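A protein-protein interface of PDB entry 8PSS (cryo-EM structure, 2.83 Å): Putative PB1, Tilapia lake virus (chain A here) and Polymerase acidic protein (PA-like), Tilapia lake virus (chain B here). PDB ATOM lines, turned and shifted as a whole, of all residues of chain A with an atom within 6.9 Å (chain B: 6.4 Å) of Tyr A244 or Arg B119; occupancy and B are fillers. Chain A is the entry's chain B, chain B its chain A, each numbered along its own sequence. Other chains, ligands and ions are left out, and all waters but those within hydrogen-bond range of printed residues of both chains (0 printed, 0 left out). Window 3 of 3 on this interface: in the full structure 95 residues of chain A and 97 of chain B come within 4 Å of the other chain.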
ATOM      1  N   LEU A 121     -21.962   9.051 -15.539  1.00  0.00           N
ATOM      2  CA  LEU A 121     -21.629   9.631 -14.243  1.00  0.00           C
ATOM      3  C   LEU A 121     -21.614   8.574 -13.148  1.00  0.00           C
ATOM      4  O   LEU A 121     -20.861   8.700 -12.175  1.00  0.00           O
ATOM      5  CB  LEU A 121     -22.625  10.737 -13.894  1.00  0.00           C
ATOM      6  CG  LEU A 121     -22.495  12.037 -14.688  1.00  0.00           C
ATOM      7  CD1 LEU A 121     -23.720  12.911 -14.478  1.00  0.00           C
ATOM      8  CD2 LEU A 121     -21.232  12.783 -14.295  1.00  0.00           C
ATOM      9  N   GLU A 131     -20.110  11.155 -10.367  1.00  0.00           N
ATOM     10  CA  GLU A 131     -21.210  11.791  -9.651  1.00  0.00           C
ATOM     11  C   GLU A 131     -20.834  12.060  -8.199  1.00  0.00           C
ATOM     12  O   GLU A 131     -21.094  13.149  -7.672  1.00  0.00           O
ATOM     13  CB  GLU A 131     -22.458  10.911  -9.731  1.00  0.00           C
ATOM     14  CG  GLU A 131     -23.691  11.513  -9.079  1.00  0.00           C
ATOM     15  CD  GLU A 131     -24.345  12.568  -9.944  1.00  0.00           C
ATOM     16  OE1 GLU A 131     -24.715  12.251 -11.094  1.00  0.00           O
ATOM     17  OE2 GLU A 131     -24.487  13.717  -9.476  1.00  0.00           O
ATOM     18  N   LEU A 134     -18.361  14.961  -8.043  1.00  0.00           N
ATOM     19  CA  LEU A 134     -18.998  16.261  -8.222  1.00  0.00           C
ATOM     20  C   LEU A 134     -19.820  16.643  -6.999  1.00  0.00           C
ATOM     21  O   LEU A 134     -19.885  17.822  -6.632  1.00  0.00           O
ATOM     22  CB  LEU A 134     -19.873  16.249  -9.474  1.00  0.00           C
ATOM     23  CG  LEU A 134     -19.146  16.154 -10.818  1.00  0.00           C
ATOM     24  CD1 LEU A 134     -20.158  16.073 -11.945  1.00  0.00           C
ATOM     25  CD2 LEU A 134     -18.199  17.326 -11.039  1.00  0.00           C
ATOM     26  N   SER A 135     -20.465  15.665  -6.362  1.00  0.00           N
ATOM     27  CA  SER A 135     -21.208  15.953  -5.142  1.00  0.00           C
ATOM     28  C   SER A 135     -20.277  16.425  -4.032  1.00  0.00           C
ATOM     29  O   SER A 135     -20.599  17.365  -3.296  1.00  0.00           O
ATOM     30  CB  SER A 135     -21.984  14.715  -4.699  1.00  0.00           C
ATOM     31  OG  SER A 135     -22.351  14.806  -3.334  1.00  0.00           O
ATOM     32  N   ARG A 138     -18.409  20.218  -4.220  1.00  0.00           N
ATOM     33  CA  ARG A 138     -19.178  21.438  -4.026  1.00  0.00           C
ATOM     34  C   ARG A 138     -19.185  21.913  -2.579  1.00  0.00           C
ATOM     35  O   ARG A 138     -19.843  22.912  -2.274  1.00  0.00           O
ATOM     36  CB  ARG A 138     -20.618  21.227  -4.501  1.00  0.00           C
ATOM     37  CG  ARG A 138     -21.493  20.495  -3.502  1.00  0.00           C
ATOM     38  CD  ARG A 138     -22.671  19.828  -4.184  1.00  0.00           C
ATOM     39  NE  ARG A 138     -23.561  19.186  -3.224  1.00  0.00           N
ATOM     40  CZ  ARG A 138     -24.505  19.814  -2.539  1.00  0.00           C
ATOM     41  NH1 ARG A 138     -24.711  21.115  -2.674  1.00  0.00           N
ATOM     42  NH2 ARG A 138     -25.264  19.121  -1.695  1.00  0.00           N
ATOM     43  N   ALA A 223     -21.674  31.705 -11.924  1.00  0.00           N
ATOM     44  CA  ALA A 223     -21.209  30.520 -12.632  1.00  0.00           C
ATOM     45  C   ALA A 223     -21.504  30.614 -14.122  1.00  0.00           C
ATOM     46  O   ALA A 223     -20.766  30.050 -14.938  1.00  0.00           O
ATOM     47  CB  ALA A 223     -21.859  29.268 -12.042  1.00  0.00           C
ATOM     48  N   LEU A 227     -18.799  29.892 -17.065  1.00  0.00           N
ATOM     49  CA  LEU A 227     -19.036  28.926 -18.131  1.00  0.00           C
ATOM     50  C   LEU A 227     -18.973  29.592 -19.498  1.00  0.00           C
ATOM     51  O   LEU A 227     -18.458  29.007 -20.455  1.00  0.00           O
ATOM     52  CB  LEU A 227     -20.389  28.243 -17.933  1.00  0.00           C
ATOM     53  CG  LEU A 227     -20.687  27.071 -18.872  1.00  0.00           C
ATOM     54  CD1 LEU A 227     -19.614  26.000 -18.777  1.00  0.00           C
ATOM     55  CD2 LEU A 227     -22.055  26.486 -18.570  1.00  0.00           C
ATOM     56  N   TRP A 230     -15.293  30.082 -20.271  1.00  0.00           N
ATOM     57  CA  TRP A 230     -14.633  28.804 -20.515  1.00  0.00           C
ATOM     58  C   TRP A 230     -15.028  28.226 -21.867  1.00  0.00           C
ATOM     59  O   TRP A 230     -14.183  27.684 -22.587  1.00  0.00           O
ATOM     60  CB  TRP A 230     -14.964  27.830 -19.385  1.00  0.00           C
ATOM     61  CG  TRP A 230     -14.397  28.252 -18.066  1.00  0.00           C
ATOM     62  CD1 TRP A 230     -13.292  29.023 -17.860  1.00  0.00           C
ATOM     63  CD2 TRP A 230     -14.910  27.934 -16.768  1.00  0.00           C
ATOM     64  NE1 TRP A 230     -13.085  29.205 -16.517  1.00  0.00           N
ATOM     65  CE2 TRP A 230     -14.065  28.546 -15.824  1.00  0.00           C
ATOM     66  CE3 TRP A 230     -16.001  27.190 -16.312  1.00  0.00           C
ATOM     67  CZ2 TRP A 230     -14.274  28.437 -14.452  1.00  0.00           C
ATOM     68  CZ3 TRP A 230     -16.209  27.085 -14.950  1.00  0.00           C
ATOM     69  CH2 TRP A 230     -15.350  27.704 -14.037  1.00  0.00           C
ATOM     70  N   ILE A 238     -14.548  20.108 -18.789  1.00  0.00           N
ATOM     71  CA  ILE A 238     -13.970  20.566 -17.527  1.00  0.00           C
ATOM     72  C   ILE A 238     -14.666  21.840 -17.064  1.00  0.00           C
ATOM     73  O   ILE A 238     -15.020  21.987 -15.888  1.00  0.00           O
ATOM     74  CB  ILE A 238     -12.452  20.773 -17.676  1.00  0.00           C
ATOM     75  CG1 ILE A 238     -11.720  19.439 -17.541  1.00  0.00           C
ATOM     76  CG2 ILE A 238     -11.933  21.752 -16.632  1.00  0.00           C
ATOM     77  CD1 ILE A 238     -10.390  19.404 -18.258  1.00  0.00           C
ATOM     78  N   GLY A 239     -14.871  22.780 -17.986  1.00  0.00           N
ATOM     79  CA  GLY A 239     -15.569  24.004 -17.636  1.00  0.00           C
ATOM     80  C   GLY A 239     -16.998  23.750 -17.199  1.00  0.00           C
ATOM     81  O   GLY A 239     -17.488  24.370 -16.254  1.00  0.00           O
ATOM     82  N   VAL A 240     -17.687  22.837 -17.884  1.00  0.00           N
ATOM     83  CA  VAL A 240     -19.061  22.509 -17.511  1.00  0.00           C
ATOM     84  C   VAL A 240     -19.098  21.930 -16.104  1.00  0.00           C
ATOM     85  O   VAL A 240     -19.951  22.290 -15.285  1.00  0.00           O
ATOM     86  CB  VAL A 240     -19.678  21.540 -18.535  1.00  0.00           C
ATOM     87  CG1 VAL A 240     -21.046  21.072 -18.067  1.00  0.00           C
ATOM     88  CG2 VAL A 240     -19.774  22.199 -19.900  1.00  0.00           C
ATOM     89  N   MET A 241     -18.175  21.014 -15.806  1.00  0.00           N
ATOM     90  CA  MET A 241     -18.141  20.404 -14.481  1.00  0.00           C
ATOM     91  C   MET A 241     -17.850  21.444 -13.407  1.00  0.00           C
ATOM     92  O   MET A 241     -18.477  21.442 -12.341  1.00  0.00           O
ATOM     93  CB  MET A 241     -17.092  19.294 -14.447  1.00  0.00           C
ATOM     94  CG  MET A 241     -17.680  17.894 -14.504  1.00  0.00           C
ATOM     95  SD  MET A 241     -16.453  16.569 -14.476  1.00  0.00           S
ATOM     96  CE  MET A 241     -15.216  17.187 -15.611  1.00  0.00           C
ATOM     97  N   LEU A 242     -16.896  22.342 -13.670  1.00  0.00           N
ATOM     98  CA  LEU A 242     -16.580  23.382 -12.697  1.00  0.00           C
ATOM     99  C   LEU A 242     -17.767  24.309 -12.474  1.00  0.00           C
ATOM    100  O   LEU A 242     -18.060  24.688 -11.335  1.00  0.00           O
ATOM    101  CB  LEU A 242     -15.361  24.178 -13.156  1.00  0.00           C
ATOM    102  CG  LEU A 242     -14.025  23.714 -12.574  1.00  0.00           C
ATOM    103  CD1 LEU A 242     -12.878  24.337 -13.339  1.00  0.00           C
ATOM    104  CD2 LEU A 242     -13.932  24.057 -11.096  1.00  0.00           C
ATOM    105  N   ALA A 243     -18.459  24.692 -13.549  1.00  0.00           N
ATOM    106  CA  ALA A 243     -19.631  25.547 -13.402  1.00  0.00           C
ATOM    107  C   ALA A 243     -20.721  24.846 -12.603  1.00  0.00           C
ATOM    108  O   ALA A 243     -21.371  25.462 -11.751  1.00  0.00           O
ATOM    109  CB  ALA A 243     -20.155  25.959 -14.776  1.00  0.00           C
ATOM    110  N   TYR A 244     -20.935  23.556 -12.866  1.00  0.00           N
ATOM    111  CA  TYR A 244     -21.935  22.807 -12.115  1.00  0.00           C
ATOM    112  C   TYR A 244     -21.580  22.749 -10.636  1.00  0.00           C
ATOM    113  O   TYR A 244     -22.450  22.905  -9.773  1.00  0.00           O
ATOM    114  CB  TYR A 244     -22.070  21.399 -12.692  1.00  0.00           C
ATOM    115  CG  TYR A 244     -23.092  20.540 -11.987  1.00  0.00           C
ATOM    116  CD1 TYR A 244     -24.443  20.850 -12.042  1.00  0.00           C
ATOM    117  CD2 TYR A 244     -22.708  19.418 -11.270  1.00  0.00           C
ATOM    118  CE1 TYR A 244     -25.381  20.069 -11.399  1.00  0.00           C
ATOM    119  CE2 TYR A 244     -23.638  18.630 -10.624  1.00  0.00           C
ATOM    120  CZ  TYR A 244     -24.973  18.960 -10.693  1.00  0.00           C
ATOM    121  OH  TYR A 244     -25.905  18.177 -10.052  1.00  0.00           O
ATOM    122  N   MET A 245     -20.302  22.525 -10.323  1.00  0.00           N
ATOM    123  CA  MET A 245     -19.887  22.481  -8.925  1.00  0.00           C
ATOM    124  C   MET A 245     -20.041  23.843  -8.259  1.00  0.00           C
ATOM    125  O   MET A 245     -20.440  23.929  -7.093  1.00  0.00           O
ATOM    126  CB  MET A 245     -18.443  21.992  -8.819  1.00  0.00           C
ATOM    127  CG  MET A 245     -18.322  20.499  -8.558  1.00  0.00           C
ATOM    128  SD  MET A 245     -16.631  19.968  -8.237  1.00  0.00           S
ATOM    129  CE  MET A 245     -15.872  20.252  -9.829  1.00  0.00           C
ATOM    130  N   VAL A 246     -19.726  24.920  -8.982  1.00  0.00           N
ATOM    131  CA  VAL A 246     -19.829  26.256  -8.404  1.00  0.00           C
ATOM    132  C   VAL A 246     -21.288  26.624  -8.160  1.00  0.00           C
ATOM    133  O   VAL A 246     -21.617  27.280  -7.165  1.00  0.00           O
ATOM    134  CB  VAL A 246     -19.133  27.285  -9.313  1.00  0.00           C
ATOM    135  CG1 VAL A 246     -19.459  28.700  -8.862  1.00  0.00           C
ATOM    136  CG2 VAL A 246     -17.632  27.062  -9.316  1.00  0.00           C
ATOM    137  N   ARG A 247     -22.183  26.217  -9.061  1.00  0.00           N
ATOM    138  CA  ARG A 247     -23.587  26.587  -8.920  1.00  0.00           C
ATOM    139  C   ARG A 247     -24.219  25.946  -7.691  1.00  0.00           C
ATOM    140  O   ARG A 247     -25.103  26.546  -7.070  1.00  0.00           O
ATOM    141  CB  ARG A 247     -24.357  26.196 -10.182  1.00  0.00           C
ATOM    142  CG  ARG A 247     -25.867  26.403 -10.103  1.00  0.00           C
ATOM    143  CD  ARG A 247     -26.236  27.870  -9.952  1.00  0.00           C
ATOM    144  NE  ARG A 247     -26.092  28.597 -11.209  1.00  0.00           N
ATOM    145  CZ  ARG A 247     -25.751  29.875 -11.309  1.00  0.00           C
ATOM    146  NH1 ARG A 247     -25.504  30.613 -10.240  1.00  0.00           N
ATOM    147  NH2 ARG A 247     -25.656  30.427 -12.515  1.00  0.00           N
ATOM    148  N   ARG A 248     -23.791  24.739  -7.325  1.00  0.00           N
ATOM    149  CA  ARG A 248     -24.377  23.996  -6.218  1.00  0.00           C
ATOM    150  C   ARG A 248     -23.518  24.038  -4.961  1.00  0.00           C
ATOM    151  O   ARG A 248     -23.709  23.216  -4.059  1.00  0.00           O
ATOM    152  CB  ARG A 248     -24.614  22.543  -6.629  1.00  0.00           C
ATOM    153  CG  ARG A 248     -25.416  22.384  -7.913  1.00  0.00           C
ATOM    154  CD  ARG A 248     -26.058  21.007  -8.039  1.00  0.00           C
ATOM    155  NE  ARG A 248     -26.608  20.517  -6.779  1.00  0.00           N
ATOM    156  CZ  ARG A 248     -26.413  19.303  -6.280  1.00  0.00           C
ATOM    157  NH1 ARG A 248     -25.682  18.398  -6.913  1.00  0.00           N
ATOM    158  NH2 ARG A 248     -26.967  18.986  -5.114  1.00  0.00           N
ATOM    159  N   LYS A 249     -22.579  24.976  -4.877  1.00  0.00           N
ATOM    160  CA  LYS A 249     -21.626  24.977  -3.779  1.00  0.00           C
ATOM    161  C   LYS A 249     -22.322  25.210  -2.443  1.00  0.00           C
ATOM    162  O   LYS A 249     -23.305  25.949  -2.345  1.00  0.00           O
ATOM    163  CB  LYS A 249     -20.558  26.047  -4.002  1.00  0.00           C
ATOM    164  CG  LYS A 249     -21.086  27.468  -4.003  1.00  0.00           C
ATOM    165  CD  LYS A 249     -20.080  28.418  -4.624  1.00  0.00           C
ATOM    166  CE  LYS A 249     -20.636  29.823  -4.733  1.00  0.00           C
ATOM    167  NZ  LYS A 249     -21.635  29.936  -5.824  1.00  0.00           N
ATOM    168  N   ALA B 114     -23.888  16.705 -22.029  1.00  0.00           N
ATOM    169  CA  ALA B 114     -25.269  17.128 -22.236  1.00  0.00           C
ATOM    170  C   ALA B 114     -26.067  17.067 -20.940  1.00  0.00           C
ATOM    171  O   ALA B 114     -26.843  17.981 -20.637  1.00  0.00           O
ATOM    172  CB  ALA B 114     -25.926  16.261 -23.310  1.00  0.00           C
ATOM    173  N   GLU B 115     -25.895  15.995 -20.165  1.00  0.00           N
ATOM    174  CA  GLU B 115     -26.640  15.857 -18.918  1.00  0.00           C
ATOM    175  C   GLU B 115     -26.276  16.965 -17.939  1.00  0.00           C
ATOM    176  O   GLU B 115     -27.154  17.567 -17.306  1.00  0.00           O
ATOM    177  CB  GLU B 115     -26.373  14.484 -18.305  1.00  0.00           C
ATOM    178  CG  GLU B 115     -27.241  14.161 -17.101  1.00  0.00           C
ATOM    179  CD  GLU B 115     -26.896  12.823 -16.481  1.00  0.00           C
ATOM    180  OE1 GLU B 115     -25.880  12.224 -16.890  1.00  0.00           O
ATOM    181  OE2 GLU B 115     -27.641  12.370 -15.587  1.00  0.00           O
ATOM    182  N   LEU B 116     -24.980  17.249 -17.797  1.00  0.00           N
ATOM    183  CA  LEU B 116     -24.554  18.300 -16.880  1.00  0.00           C
ATOM    184  C   LEU B 116     -25.044  19.665 -17.344  1.00  0.00           C
ATOM    185  O   LEU B 116     -25.448  20.498 -16.524  1.00  0.00           O
ATOM    186  CB  LEU B 116     -23.032  18.293 -16.745  1.00  0.00           C
ATOM    187  CG  LEU B 116     -22.418  17.153 -15.926  1.00  0.00           C
ATOM    188  CD1 LEU B 116     -20.921  17.356 -15.787  1.00  0.00           C
ATOM    189  CD2 LEU B 116     -23.068  17.037 -14.555  1.00  0.00           C
ATOM    190  N   ARG B 117     -25.013  19.916 -18.654  1.00  0.00           N
ATOM    191  CA  ARG B 117     -25.513  21.188 -19.165  1.00  0.00           C
ATOM    192  C   ARG B 117     -27.007  21.334 -18.904  1.00  0.00           C
ATOM    193  O   ARG B 117     -27.476  22.414 -18.527  1.00  0.00           O
ATOM    194  CB  ARG B 117     -25.208  21.307 -20.656  1.00  0.00           C
ATOM    195  CG  ARG B 117     -23.753  21.624 -20.952  1.00  0.00           C
ATOM    196  CD  ARG B 117     -23.544  22.006 -22.403  1.00  0.00           C
ATOM    197  NE  ARG B 117     -22.131  22.189 -22.715  1.00  0.00           N
ATOM    198  CZ  ARG B 117     -21.452  23.309 -22.502  1.00  0.00           C
ATOM    199  NH1 ARG B 117     -22.026  24.376 -21.972  1.00  0.00           N
ATOM    200  NH2 ARG B 117     -20.164  23.357 -22.828  1.00  0.00           N
ATOM    201  N   GLU B 118     -27.770  20.257 -19.093  1.00  0.00           N
ATOM    202  CA  GLU B 118     -29.196  20.308 -18.791  1.00  0.00           C
ATOM    203  C   GLU B 118     -29.430  20.574 -17.310  1.00  0.00           C
ATOM    204  O   GLU B 118     -30.282  21.393 -16.943  1.00  0.00           O
ATOM    205  CB  GLU B 118     -29.868  19.003 -19.217  1.00  0.00           C
ATOM    206  CG  GLU B 118     -31.355  18.932 -18.886  1.00  0.00           C
ATOM    207  CD  GLU B 118     -31.675  17.974 -17.751  1.00  0.00           C
ATOM    208  OE1 GLU B 118     -30.835  17.106 -17.433  1.00  0.00           O
ATOM    209  OE2 GLU B 118     -32.775  18.093 -17.170  1.00  0.00           O
ATOM    210  N   ARG B 119     -28.673  19.899 -16.441  1.00  0.00           N
ATOM    211  CA  ARG B 119     -28.823  20.122 -15.006  1.00  0.00           C
ATOM    212  C   ARG B 119     -28.512  21.568 -14.645  1.00  0.00           C
ATOM    213  O   ARG B 119     -29.212  22.177 -13.828  1.00  0.00           O
ATOM    214  CB  ARG B 119     -27.919  19.169 -14.227  1.00  0.00           C
ATOM    215  CG  ARG B 119     -28.524  17.791 -14.008  1.00  0.00           C
ATOM    216  CD  ARG B 119     -27.507  16.679 -14.209  1.00  0.00           C
ATOM    217  NE  ARG B 119     -26.719  16.448 -13.003  1.00  0.00           N
ATOM    218  CZ  ARG B 119     -26.642  15.295 -12.349  1.00  0.00           C
ATOM    219  NH1 ARG B 119     -27.289  14.216 -12.757  1.00  0.00           N
ATOM    220  NH2 ARG B 119     -25.892  15.224 -11.252  1.00  0.00           N
ATOM    221  N   LEU B 120     -27.464  22.134 -15.246  1.00  0.00           N
ATOM    222  CA  LEU B 120     -27.161  23.543 -15.026  1.00  0.00           C
ATOM    223  C   LEU B 120     -28.312  24.424 -15.491  1.00  0.00           C
ATOM    224  O   LEU B 120     -28.668  25.401 -14.822  1.00  0.00           O
ATOM    225  CB  LEU B 120     -25.874  23.923 -15.755  1.00  0.00           C
ATOM    226  CG  LEU B 120     -24.598  23.940 -14.913  1.00  0.00           C
ATOM    227  CD1 LEU B 120     -23.378  24.017 -15.813  1.00  0.00           C
ATOM    228  CD2 LEU B 120     -24.613  25.101 -13.932  1.00  0.00           C
ATOM    229  N   LEU B 121     -28.907  24.092 -16.638  1.00  0.00           N
ATOM    230  CA  LEU B 121     -30.024  24.881 -17.145  1.00  0.00           C
ATOM    231  C   LEU B 121     -31.199  24.861 -16.176  1.00  0.00           C
ATOM    232  O   LEU B 121     -31.839  25.894 -15.946  1.00  0.00           O
ATOM    233  CB  LEU B 121     -30.453  24.356 -18.516  1.00  0.00           C
ATOM    234  CG  LEU B 121     -31.184  25.326 -19.450  1.00  0.00           C
ATOM    235  CD1 LEU B 121     -30.441  26.647 -19.593  1.00  0.00           C
ATOM    236  CD2 LEU B 121     -31.395  24.682 -20.811  1.00  0.00           C
ATOM    237  N   GLU B 122     -31.502  23.698 -15.596  1.00  0.00           N
ATOM    238  CA  GLU B 122     -32.621  23.613 -14.664  1.00  0.00           C
ATOM    239  C   GLU B 122     -32.345  24.310 -13.337  1.00  0.00           C
ATOM    240  O   GLU B 122     -33.281  24.496 -12.553  1.00  0.00           O
ATOM    241  CB  GLU B 122     -32.989  22.152 -14.390  1.00  0.00           C
ATOM    242  CG  GLU B 122     -33.108  21.260 -15.623  1.00  0.00           C
ATOM    243  CD  GLU B 122     -33.707  21.965 -16.828  1.00  0.00           C
ATOM    244  OE1 GLU B 122     -33.354  21.594 -17.967  1.00  0.00           O
ATOM    245  OE2 GLU B 122     -34.547  22.871 -16.643  1.00  0.00           O
ATOM    246  N   LEU B 123     -31.106  24.692 -13.063  1.00  0.00           N
ATOM    247  CA  LEU B 123     -30.750  25.329 -11.803  1.00  0.00           C
ATOM    248  C   LEU B 123     -31.020  26.824 -11.871  1.00  0.00           C
ATOM    249  O   LEU B 123     -31.179  27.399 -12.949  1.00  0.00           O
ATOM    250  CB  LEU B 123     -29.285  25.047 -11.481  1.00  0.00           C
ATOM    251  CG  LEU B 123     -29.016  23.665 -10.880  1.00  0.00           C
ATOM    252  CD1 LEU B 123     -27.533  23.339 -10.917  1.00  0.00           C
ATOM    253  CD2 LEU B 123     -29.543  23.583  -9.456  1.00  0.00           C
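The side-chain carboxylate of Glu A131 is in salt-bridge range of the guanidinium group of Arg B119 (2.7 Å). The side-chain hydroxyl of Tyr A244 lies within hydrogen-bond range of the guanidinium group of Arg B119.
The guanidinium group (NH1) of Arg A138 lies within hydrogen-bond range of the backbone carbonyl oxygen (O) of Arg A248 (2.7 Å). NH1 of Arg A248 is in hydrogen-bond range of OH of Tyr A244, at 3.2 Å. The backbone NH (N) of Glu A131 lies within hydrogen-bond range of the backbone carbonyl oxygen (O) of Leu A121. The guanidinium group (NH1) of Arg B119 is in salt-bridge range of the side-chain carboxylate (OE2) of Glu B115.
Among the printed residues, pairs that only touch across the chains: Leu A121 with Glu B115 (3.3 Å), Leu A227 with Leu B120 (3.9 Å), Val A240 with Leu B116 (3.7 Å), Val A240 with Arg B117 (3.2 Å), Val A240 with Leu B120 (3.9 Å), Met A241 with Leu B116 (3.5 Å), Ala A243 with Leu B120 (3.9 Å), Tyr A244 with Leu B120 (3.9 Å), Tyr A244 with Leu B123 (3.9 Å), Arg A247 with Leu B120 (3.9 Å), Arg A247 with Leu B123 (3.6 Å) and Arg A248 with Leu B123 (3.8 Å).
Of the printed residues of chain B, Glu A131 touches Arg B119. Of chain B, only Arg B119, Leu B120 and Leu B123 come within 4 Å of Tyr A244. Of the printed residues of chain B, Arg A248 touches Leu B123. Of the printed residues of chain A, Arg B119 touches Glu A131 (2.7 Å) and Tyr A244 (3.2 Å). The nearest residue of chain B that does not touch Tyr A244 is Leu B116 (4.1 Å). The nearest residue of chain A that does not touch Arg B119 is Leu A121 (4.2 Å).
Of the 10 printed residues of chain B, 6 touch a printed residue of chain A. Hydrophobic or aromatic side chains of chain B within 4 Å of the printed part of chain A: Leu B116, Leu B120 and Leu B123. Among the printed residues, Asp or Glu carboxylates within 4 Å of a Lys or Arg side-chain nitrogen of the other chain: Glu A131 with Arg B119 (2.7 Å).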
